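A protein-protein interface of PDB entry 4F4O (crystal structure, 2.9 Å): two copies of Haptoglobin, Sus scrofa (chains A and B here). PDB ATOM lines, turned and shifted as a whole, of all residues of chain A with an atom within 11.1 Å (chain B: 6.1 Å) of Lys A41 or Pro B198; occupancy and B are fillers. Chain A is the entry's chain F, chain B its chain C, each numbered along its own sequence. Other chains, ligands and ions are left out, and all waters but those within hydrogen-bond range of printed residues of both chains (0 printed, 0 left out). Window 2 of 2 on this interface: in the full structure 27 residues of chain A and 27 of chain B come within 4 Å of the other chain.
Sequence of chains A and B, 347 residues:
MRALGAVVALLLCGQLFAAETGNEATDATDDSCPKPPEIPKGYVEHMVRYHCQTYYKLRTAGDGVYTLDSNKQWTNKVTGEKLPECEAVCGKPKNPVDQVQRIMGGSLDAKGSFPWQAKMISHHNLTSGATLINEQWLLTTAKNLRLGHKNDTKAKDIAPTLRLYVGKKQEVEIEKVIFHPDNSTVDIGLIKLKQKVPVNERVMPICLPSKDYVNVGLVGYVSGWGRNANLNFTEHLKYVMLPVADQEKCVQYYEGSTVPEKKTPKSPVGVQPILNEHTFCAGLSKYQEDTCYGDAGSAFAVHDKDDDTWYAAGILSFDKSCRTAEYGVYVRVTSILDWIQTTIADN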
ATOM      1  N   PRO A  37      -9.674 -19.623   9.541  1.00  0.00           N
ATOM      2  CA  PRO A  37      -8.550 -19.201  10.386  1.00  0.00           C
ATOM      3  C   PRO A  37      -7.497 -20.288  10.500  1.00  0.00           C
ATOM      4  O   PRO A  37      -7.771 -21.466  10.219  1.00  0.00           O
ATOM      5  CB  PRO A  37      -9.203 -18.960  11.743  1.00  0.00           C
ATOM      6  CG  PRO A  37     -10.406 -19.845  11.728  1.00  0.00           C
ATOM      7  CD  PRO A  37     -10.902 -19.848  10.317  1.00  0.00           C
ATOM      8  N   GLU A  38      -6.294 -19.887  10.909  1.00  0.00           N
ATOM      9  CA  GLU A  38      -5.198 -20.828  11.017  1.00  0.00           C
ATOM     10  C   GLU A  38      -4.956 -21.382  12.417  1.00  0.00           C
ATOM     11  O   GLU A  38      -5.009 -20.673  13.425  1.00  0.00           O
ATOM     12  CB  GLU A  38      -3.916 -20.268  10.402  1.00  0.00           C
ATOM     13  CG  GLU A  38      -3.597 -20.879   9.040  1.00  0.00           C
ATOM     14  CD  GLU A  38      -4.315 -22.223   8.819  1.00  0.00           C
ATOM     15  OE1 GLU A  38      -3.994 -23.207   9.554  1.00  0.00           O
ATOM     16  OE2 GLU A  38      -5.203 -22.283   7.915  1.00  0.00           O
ATOM     17  N   ILE A  39      -4.743 -22.687  12.449  1.00  0.00           N
ATOM     18  CA  ILE A  39      -4.296 -23.389  13.639  1.00  0.00           C
ATOM     19  C   ILE A  39      -2.747 -23.545  13.669  1.00  0.00           C
ATOM     20  O   ILE A  39      -2.100 -23.786  12.633  1.00  0.00           O
ATOM     21  CB  ILE A  39      -4.979 -24.760  13.718  1.00  0.00           C
ATOM     22  CG1 ILE A  39      -6.031 -24.793  14.811  1.00  0.00           C
ATOM     23  CG2 ILE A  39      -4.009 -25.835  14.059  1.00  0.00           C
ATOM     24  CD1 ILE A  39      -6.471 -26.209  15.064  1.00  0.00           C
ATOM     25  N   PRO A  40      -2.127 -23.382  14.848  1.00  0.00           N
ATOM     26  CA  PRO A  40      -0.709 -23.746  14.839  1.00  0.00           C
ATOM     27  C   PRO A  40      -0.562 -25.275  14.826  1.00  0.00           C
ATOM     28  O   PRO A  40      -1.324 -25.976  15.514  1.00  0.00           O
ATOM     29  CB  PRO A  40      -0.179 -23.112  16.128  1.00  0.00           C
ATOM     30  CG  PRO A  40      -1.362 -22.998  17.023  1.00  0.00           C
ATOM     31  CD  PRO A  40      -2.560 -22.816  16.138  1.00  0.00           C
ATOM     32  N   LYS A  41       0.398 -25.764  14.037  1.00  0.00           N
ATOM     33  CA  LYS A  41       0.644 -27.198  13.837  1.00  0.00           C
ATOM     34  C   LYS A  41      -0.525 -27.982  13.236  1.00  0.00           C
ATOM     35  O   LYS A  41      -0.632 -29.187  13.465  1.00  0.00           O
ATOM     36  CB  LYS A  41       1.080 -27.874  15.137  1.00  0.00           C
ATOM     37  CG  LYS A  41       2.359 -27.317  15.731  1.00  0.00           C
ATOM     38  CD  LYS A  41       3.537 -27.558  14.823  1.00  0.00           C
ATOM     39  CE  LYS A  41       4.755 -26.863  15.362  1.00  0.00           C
ATOM     40  NZ  LYS A  41       5.924 -27.063  14.472  1.00  0.00           N
ATOM     41  N   GLY A  42      -1.391 -27.323  12.467  1.00  0.00           N
ATOM     42  CA  GLY A  42      -2.518 -28.026  11.873  1.00  0.00           C
ATOM     43  C   GLY A  42      -3.052 -27.450  10.575  1.00  0.00           C
ATOM     44  O   GLY A  42      -2.888 -26.270  10.287  1.00  0.00           O
ATOM     45  N   TYR A  43      -3.710 -28.286   9.789  1.00  0.00           N
ATOM     46  CA  TYR A  43      -4.146 -27.866   8.470  1.00  0.00           C
ATOM     47  C   TYR A  43      -5.660 -28.056   8.270  1.00  0.00           C
ATOM     48  O   TYR A  43      -6.300 -28.858   8.960  1.00  0.00           O
ATOM     49  CB  TYR A  43      -3.360 -28.625   7.406  1.00  0.00           C
ATOM     50  CG  TYR A  43      -3.491 -30.122   7.533  1.00  0.00           C
ATOM     51  CD1 TYR A  43      -4.497 -30.809   6.866  1.00  0.00           C
ATOM     52  CD2 TYR A  43      -2.614 -30.850   8.319  1.00  0.00           C
ATOM     53  CE1 TYR A  43      -4.630 -32.179   6.979  1.00  0.00           C
ATOM     54  CE2 TYR A  43      -2.737 -32.230   8.436  1.00  0.00           C
ATOM     55  CZ  TYR A  43      -3.752 -32.884   7.761  1.00  0.00           C
ATOM     56  OH  TYR A  43      -3.895 -34.246   7.865  1.00  0.00           O
ATOM     57  N   VAL A  44      -6.235 -27.322   7.324  1.00  0.00           N
ATOM     58  CA  VAL A  44      -7.657 -27.473   7.052  1.00  0.00           C
ATOM     59  C   VAL A  44      -7.974 -28.458   5.927  1.00  0.00           C
ATOM     60  O   VAL A  44      -7.217 -28.602   4.971  1.00  0.00           O
ATOM     61  CB  VAL A  44      -8.347 -26.120   6.767  1.00  0.00           C
ATOM     62  CG1 VAL A  44      -8.808 -25.483   8.064  1.00  0.00           C
ATOM     63  CG2 VAL A  44      -7.413 -25.190   6.019  1.00  0.00           C
ATOM     64  N   HIS B  51      -7.261 -30.777  11.064  1.00  0.00           N
ATOM     65  CA  HIS B  51      -6.466 -31.964  11.338  1.00  0.00           C
ATOM     66  C   HIS B  51      -5.112 -31.538  11.854  1.00  0.00           C
ATOM     67  O   HIS B  51      -4.672 -30.412  11.604  1.00  0.00           O
ATOM     68  CB  HIS B  51      -6.281 -32.801  10.079  1.00  0.00           C
ATOM     69  CG  HIS B  51      -7.566 -33.285   9.497  1.00  0.00           C
ATOM     70  ND1 HIS B  51      -8.284 -34.325  10.044  1.00  0.00           N
ATOM     71  CD2 HIS B  51      -8.273 -32.855   8.428  1.00  0.00           C
ATOM     72  CE1 HIS B  51      -9.377 -34.523   9.328  1.00  0.00           C
ATOM     73  NE2 HIS B  51      -9.394 -33.647   8.340  1.00  0.00           N
ATOM     74  N   CYS B  52      -4.424 -32.444  12.540  1.00  0.00           N
ATOM     75  CA  CYS B  52      -3.160 -32.082  13.140  1.00  0.00           C
ATOM     76  C   CYS B  52      -2.015 -32.722  12.400  1.00  0.00           C
ATOM     77  O   CYS B  52      -2.168 -33.769  11.768  1.00  0.00           O
ATOM     78  CB  CYS B  52      -3.136 -32.452  14.620  1.00  0.00           C
ATOM     79  SG  CYS B  52      -3.891 -31.176  15.684  1.00  0.00           S
ATOM     80  N   GLN B  53      -0.872 -32.055  12.474  1.00  0.00           N
ATOM     81  CA  GLN B  53       0.373 -32.583  11.955  1.00  0.00           C
ATOM     82  C   GLN B  53       0.649 -33.938  12.571  1.00  0.00           C
ATOM     83  O   GLN B  53       0.176 -34.259  13.660  1.00  0.00           O
ATOM     84  CB  GLN B  53       1.540 -31.626  12.261  1.00  0.00           C
ATOM     85  CG  GLN B  53       2.098 -30.943  11.029  1.00  0.00           C
ATOM     86  CD  GLN B  53       1.685 -31.682   9.742  1.00  0.00           C
ATOM     87  OE1 GLN B  53       2.296 -32.700   9.365  1.00  0.00           O
ATOM     88  NE2 GLN B  53       0.631 -31.179   9.071  1.00  0.00           N
ATOM     89  N   TYR B  56       1.190 -34.956  16.422  1.00  0.00           N
ATOM     90  CA  TYR B  56       0.255 -34.121  17.185  1.00  0.00           C
ATOM     91  C   TYR B  56      -1.180 -34.663  17.192  1.00  0.00           C
ATOM     92  O   TYR B  56      -1.540 -35.512  16.382  1.00  0.00           O
ATOM     93  CB  TYR B  56       0.239 -32.700  16.635  1.00  0.00           C
ATOM     94  CG  TYR B  56       1.512 -31.925  16.863  1.00  0.00           C
ATOM     95  CD1 TYR B  56       2.577 -32.022  15.983  1.00  0.00           C
ATOM     96  CD2 TYR B  56       1.633 -31.081  17.940  1.00  0.00           C
ATOM     97  CE1 TYR B  56       3.729 -31.304  16.184  1.00  0.00           C
ATOM     98  CE2 TYR B  56       2.773 -30.362  18.146  1.00  0.00           C
ATOM     99  CZ  TYR B  56       3.830 -30.472  17.272  1.00  0.00           C
ATOM    100  OH  TYR B  56       4.996 -29.744  17.502  1.00  0.00           O
ATOM    101  N   CYS B  86      -3.616 -28.012  18.485  1.00  0.00           N
ATOM    102  CA  CYS B  86      -2.783 -29.175  18.195  1.00  0.00           C
ATOM    103  C   CYS B  86      -1.746 -29.480  19.288  1.00  0.00           C
ATOM    104  O   CYS B  86      -0.904 -28.653  19.643  1.00  0.00           O
ATOM    105  CB  CYS B  86      -2.125 -29.024  16.833  1.00  0.00           C
ATOM    106  SG  CYS B  86      -3.339 -29.226  15.530  1.00  0.00           S
ATOM    107  N   GLU B 135       5.522 -30.298  25.628  1.00  0.00           N
ATOM    108  CA  GLU B 135       6.062 -29.355  24.647  1.00  0.00           C
ATOM    109  C   GLU B 135       6.961 -28.208  25.194  1.00  0.00           C
ATOM    110  O   GLU B 135       7.903 -27.812  24.523  1.00  0.00           O
ATOM    111  CB  GLU B 135       4.935 -28.759  23.809  1.00  0.00           C
ATOM    112  CG  GLU B 135       3.983 -29.746  23.186  1.00  0.00           C
ATOM    113  CD  GLU B 135       3.319 -29.162  21.936  1.00  0.00           C
ATOM    114  OE1 GLU B 135       4.075 -28.807  20.984  1.00  0.00           O
ATOM    115  OE2 GLU B 135       2.063 -29.036  21.915  1.00  0.00           O
ATOM    116  N   GLN B 170      20.123 -29.436  18.796  1.00  0.00           N
ATOM    117  CA  GLN B 170      19.137 -28.363  18.995  1.00  0.00           C
ATOM    118  C   GLN B 170      19.208 -27.807  20.394  1.00  0.00           C
ATOM    119  O   GLN B 170      18.910 -28.502  21.358  1.00  0.00           O
ATOM    120  CB  GLN B 170      17.710 -28.925  18.937  1.00  0.00           C
ATOM    121  CG  GLN B 170      17.148 -29.412  17.628  1.00  0.00           C
ATOM    122  CD  GLN B 170      15.615 -29.368  17.642  1.00  0.00           C
ATOM    123  OE1 GLN B 170      15.014 -28.563  18.360  1.00  0.00           O
ATOM    124  NE2 GLN B 170      14.981 -30.235  16.850  1.00  0.00           N
ATOM    125  N   LYS B 196       7.330 -23.476  23.142  1.00  0.00           N
ATOM    126  CA  LYS B 196       7.173 -24.896  22.875  1.00  0.00           C
ATOM    127  C   LYS B 196       8.208 -25.371  21.860  1.00  0.00           C
ATOM    128  O   LYS B 196       8.485 -24.648  20.886  1.00  0.00           O
ATOM    129  CB  LYS B 196       5.779 -25.161  22.303  1.00  0.00           C
ATOM    130  CG  LYS B 196       4.605 -24.664  23.129  1.00  0.00           C
ATOM    131  CD  LYS B 196       3.335 -25.306  22.571  1.00  0.00           C
ATOM    132  CE  LYS B 196       2.035 -24.683  23.089  1.00  0.00           C
ATOM    133  NZ  LYS B 196       0.850 -25.459  22.639  1.00  0.00           N
ATOM    134  N   VAL B 197       8.769 -26.571  22.085  1.00  0.00           N
ATOM    135  CA  VAL B 197       9.643 -27.222  21.096  1.00  0.00           C
ATOM    136  C   VAL B 197       8.811 -27.836  19.997  1.00  0.00           C
ATOM    137  O   VAL B 197       7.835 -28.544  20.277  1.00  0.00           O
ATOM    138  CB  VAL B 197      10.432 -28.447  21.639  1.00  0.00           C
ATOM    139  CG1 VAL B 197      11.771 -28.555  20.948  1.00  0.00           C
ATOM    140  CG2 VAL B 197      10.609 -28.388  23.106  1.00  0.00           C
ATOM    141  N   PRO B 198       9.186 -27.586  18.740  1.00  0.00           N
ATOM    142  CA  PRO B 198       8.572 -28.412  17.702  1.00  0.00           C
ATOM    143  C   PRO B 198       8.968 -29.872  17.930  1.00  0.00           C
ATOM    144  O   PRO B 198      10.146 -30.174  18.187  1.00  0.00           O
ATOM    145  CB  PRO B 198       9.156 -27.846  16.399  1.00  0.00           C
ATOM    146  CG  PRO B 198      10.355 -27.030  16.835  1.00  0.00           C
ATOM    147  CD  PRO B 198      10.020 -26.510  18.187  1.00  0.00           C
ATOM    148  N   VAL B 199       7.962 -30.744  17.866  1.00  0.00           N
ATOM    149  CA  VAL B 199       8.095 -32.182  18.077  1.00  0.00           C
ATOM    150  C   VAL B 199       8.189 -32.936  16.730  1.00  0.00           C
ATOM    151  O   VAL B 199       7.461 -32.630  15.763  1.00  0.00           O
ATOM    152  CB  VAL B 199       6.917 -32.712  18.942  1.00  0.00           C
ATOM    153  CG1 VAL B 199       6.835 -34.220  18.907  1.00  0.00           C
ATOM    154  CG2 VAL B 199       7.037 -32.217  20.371  1.00  0.00           C
ATOM    155  N   ASN B 200       9.104 -33.908  16.688  1.00  0.00           N
ATOM    156  CA  ASN B 200       9.416 -34.692  15.492  1.00  0.00           C
ATOM    157  C   ASN B 200       9.960 -36.060  15.885  1.00  0.00           C
ATOM    158  O   ASN B 200       9.800 -36.479  17.034  1.00  0.00           O
ATOM    159  CB  ASN B 200      10.414 -33.955  14.605  1.00  0.00           C
ATOM    160  CG  ASN B 200      11.421 -33.160  15.406  1.00  0.00           C
ATOM    161  OD1 ASN B 200      12.396 -33.707  15.921  1.00  0.00           O
ATOM    162  ND2 ASN B 200      11.190 -31.860  15.523  1.00  0.00           N
ATOM    163  N   VAL B 203      12.797 -35.035  18.669  1.00  0.00           N
ATOM    164  CA  VAL B 203      12.345 -34.417  19.909  1.00  0.00           C
ATOM    165  C   VAL B 203      10.892 -34.745  20.169  1.00  0.00           C
ATOM    166  O   VAL B 203      10.059 -34.504  19.314  1.00  0.00           O
ATOM    167  CB  VAL B 203      12.463 -32.887  19.826  1.00  0.00           C
ATOM    168  CG1 VAL B 203      12.041 -32.253  21.147  1.00  0.00           C
ATOM    169  CG2 VAL B 203      13.878 -32.487  19.457  1.00  0.00           C
ATOM    170  N   MET B 204      10.593 -35.269  21.350  1.00  0.00           N
ATOM    171  CA  MET B 204       9.212 -35.519  21.742  1.00  0.00           C
ATOM    172  C   MET B 204       9.137 -35.985  23.175  1.00  0.00           C
ATOM    173  O   MET B 204      10.002 -36.739  23.635  1.00  0.00           O
ATOM    174  CB  MET B 204       8.532 -36.520  20.811  1.00  0.00           C
ATOM    175  CG  MET B 204       8.363 -37.919  21.324  1.00  0.00           C
ATOM    176  SD  MET B 204       7.521 -38.944  20.087  1.00  0.00           S
ATOM    177  CE  MET B 204       5.999 -39.238  20.954  1.00  0.00           C
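The side-chain sulfur (SG) of Cys B52 is disulfide-bonded to the side-chain sulfur (SG) of Cys B86 (2.0 Å). The backbone NH (N) of Val B199 is in hydrogen-bond range of the side-chain hydroxyl (OH) of Tyr B56 (3.2 Å). ND2 of Asn B200 lies within hydrogen-bond range of O of Pro B198, at 3.3 Å.
No position is printed for both chains. Of the 12 pairs that touch across the chains among the printed residues, none has its exchanged pair printed and touching as well.
O of His B51 sits at hydrogen-bond distance from N of Tyr A43 (3.0 Å). The backbone carbonyl oxygen of Lys A41 is in hydrogen-bond range of the backbone NH of Gln B53 (3.0 Å). O of Lys A41 lies close to SG of Cys B86, 3.4 Å away.
Lys A41 touches five residues of chain B. Of the printed residues of chain B, Gly A42 touches His B51 and Cys B86. Of the printed residues of chain B, Tyr A43 touches His B51, Cys B52 and Gln B53. Val A44 touches none of the printed residues of chain B. Of chain A, only Lys A41 (3.9 Å) and Tyr A43 (3.7 Å) come within 4 Å of Cys B52. Tyr B56 touches just one residue of chain A: Lys A41. Cys B86 touches just these residues of chain A: Ile A39, Pro A40, Lys A41 and Gly A42. Glu B135 touches none of the printed residues of chain A. Pro B198 touches one residue of chain A. No residue of chain A comes within 4 Å of Val B199. No residue of chain A comes within 4 Å of Asn B200. Val B203 touches none of the printed residues of chain A. The nearest residue of chain B that does not touch Lys A41 is His B51 (4.6 Å). The nearest printed residue of chain B that does not touch Gly A42 is Cys B52 (4.3 Å).
Printed residues of chain A that touch a printed residue of chain B: Ile A39, Pro A40, Lys A41, Gly A42 and Tyr A43. Printed residues of chain B that touch a printed residue of chain A: His B51, Cys B52, Gln B53, Tyr B56, Cys B86 and Pro B198. Hydrophobic or aromatic side chains of chain B within 4 Å of the printed part of chain A: His B51, Tyr B56 and Pro B198. Among the printed residues, 12 pairs touch across the chains.
Ile A39 touches Cys B86. Pro A40 touches Cys B86. Lys A41 touches Cys B52. CE of Lys A41 touches OH of Tyr B56, 3.6 Å away. CB of Pro B198 touches NZ of Lys A41 (3.8 Å). Gly A42 touches His B51 (CA to O, 3.2 Å). CA of Gly A42 touches SG of Cys B86, at 3.9 Å. Tyr A43 touches Cys B52 (CE2 to O, 3.7 Å). Gln B53 touches Tyr A43 (NE2 to CD2, 3.3 Å).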
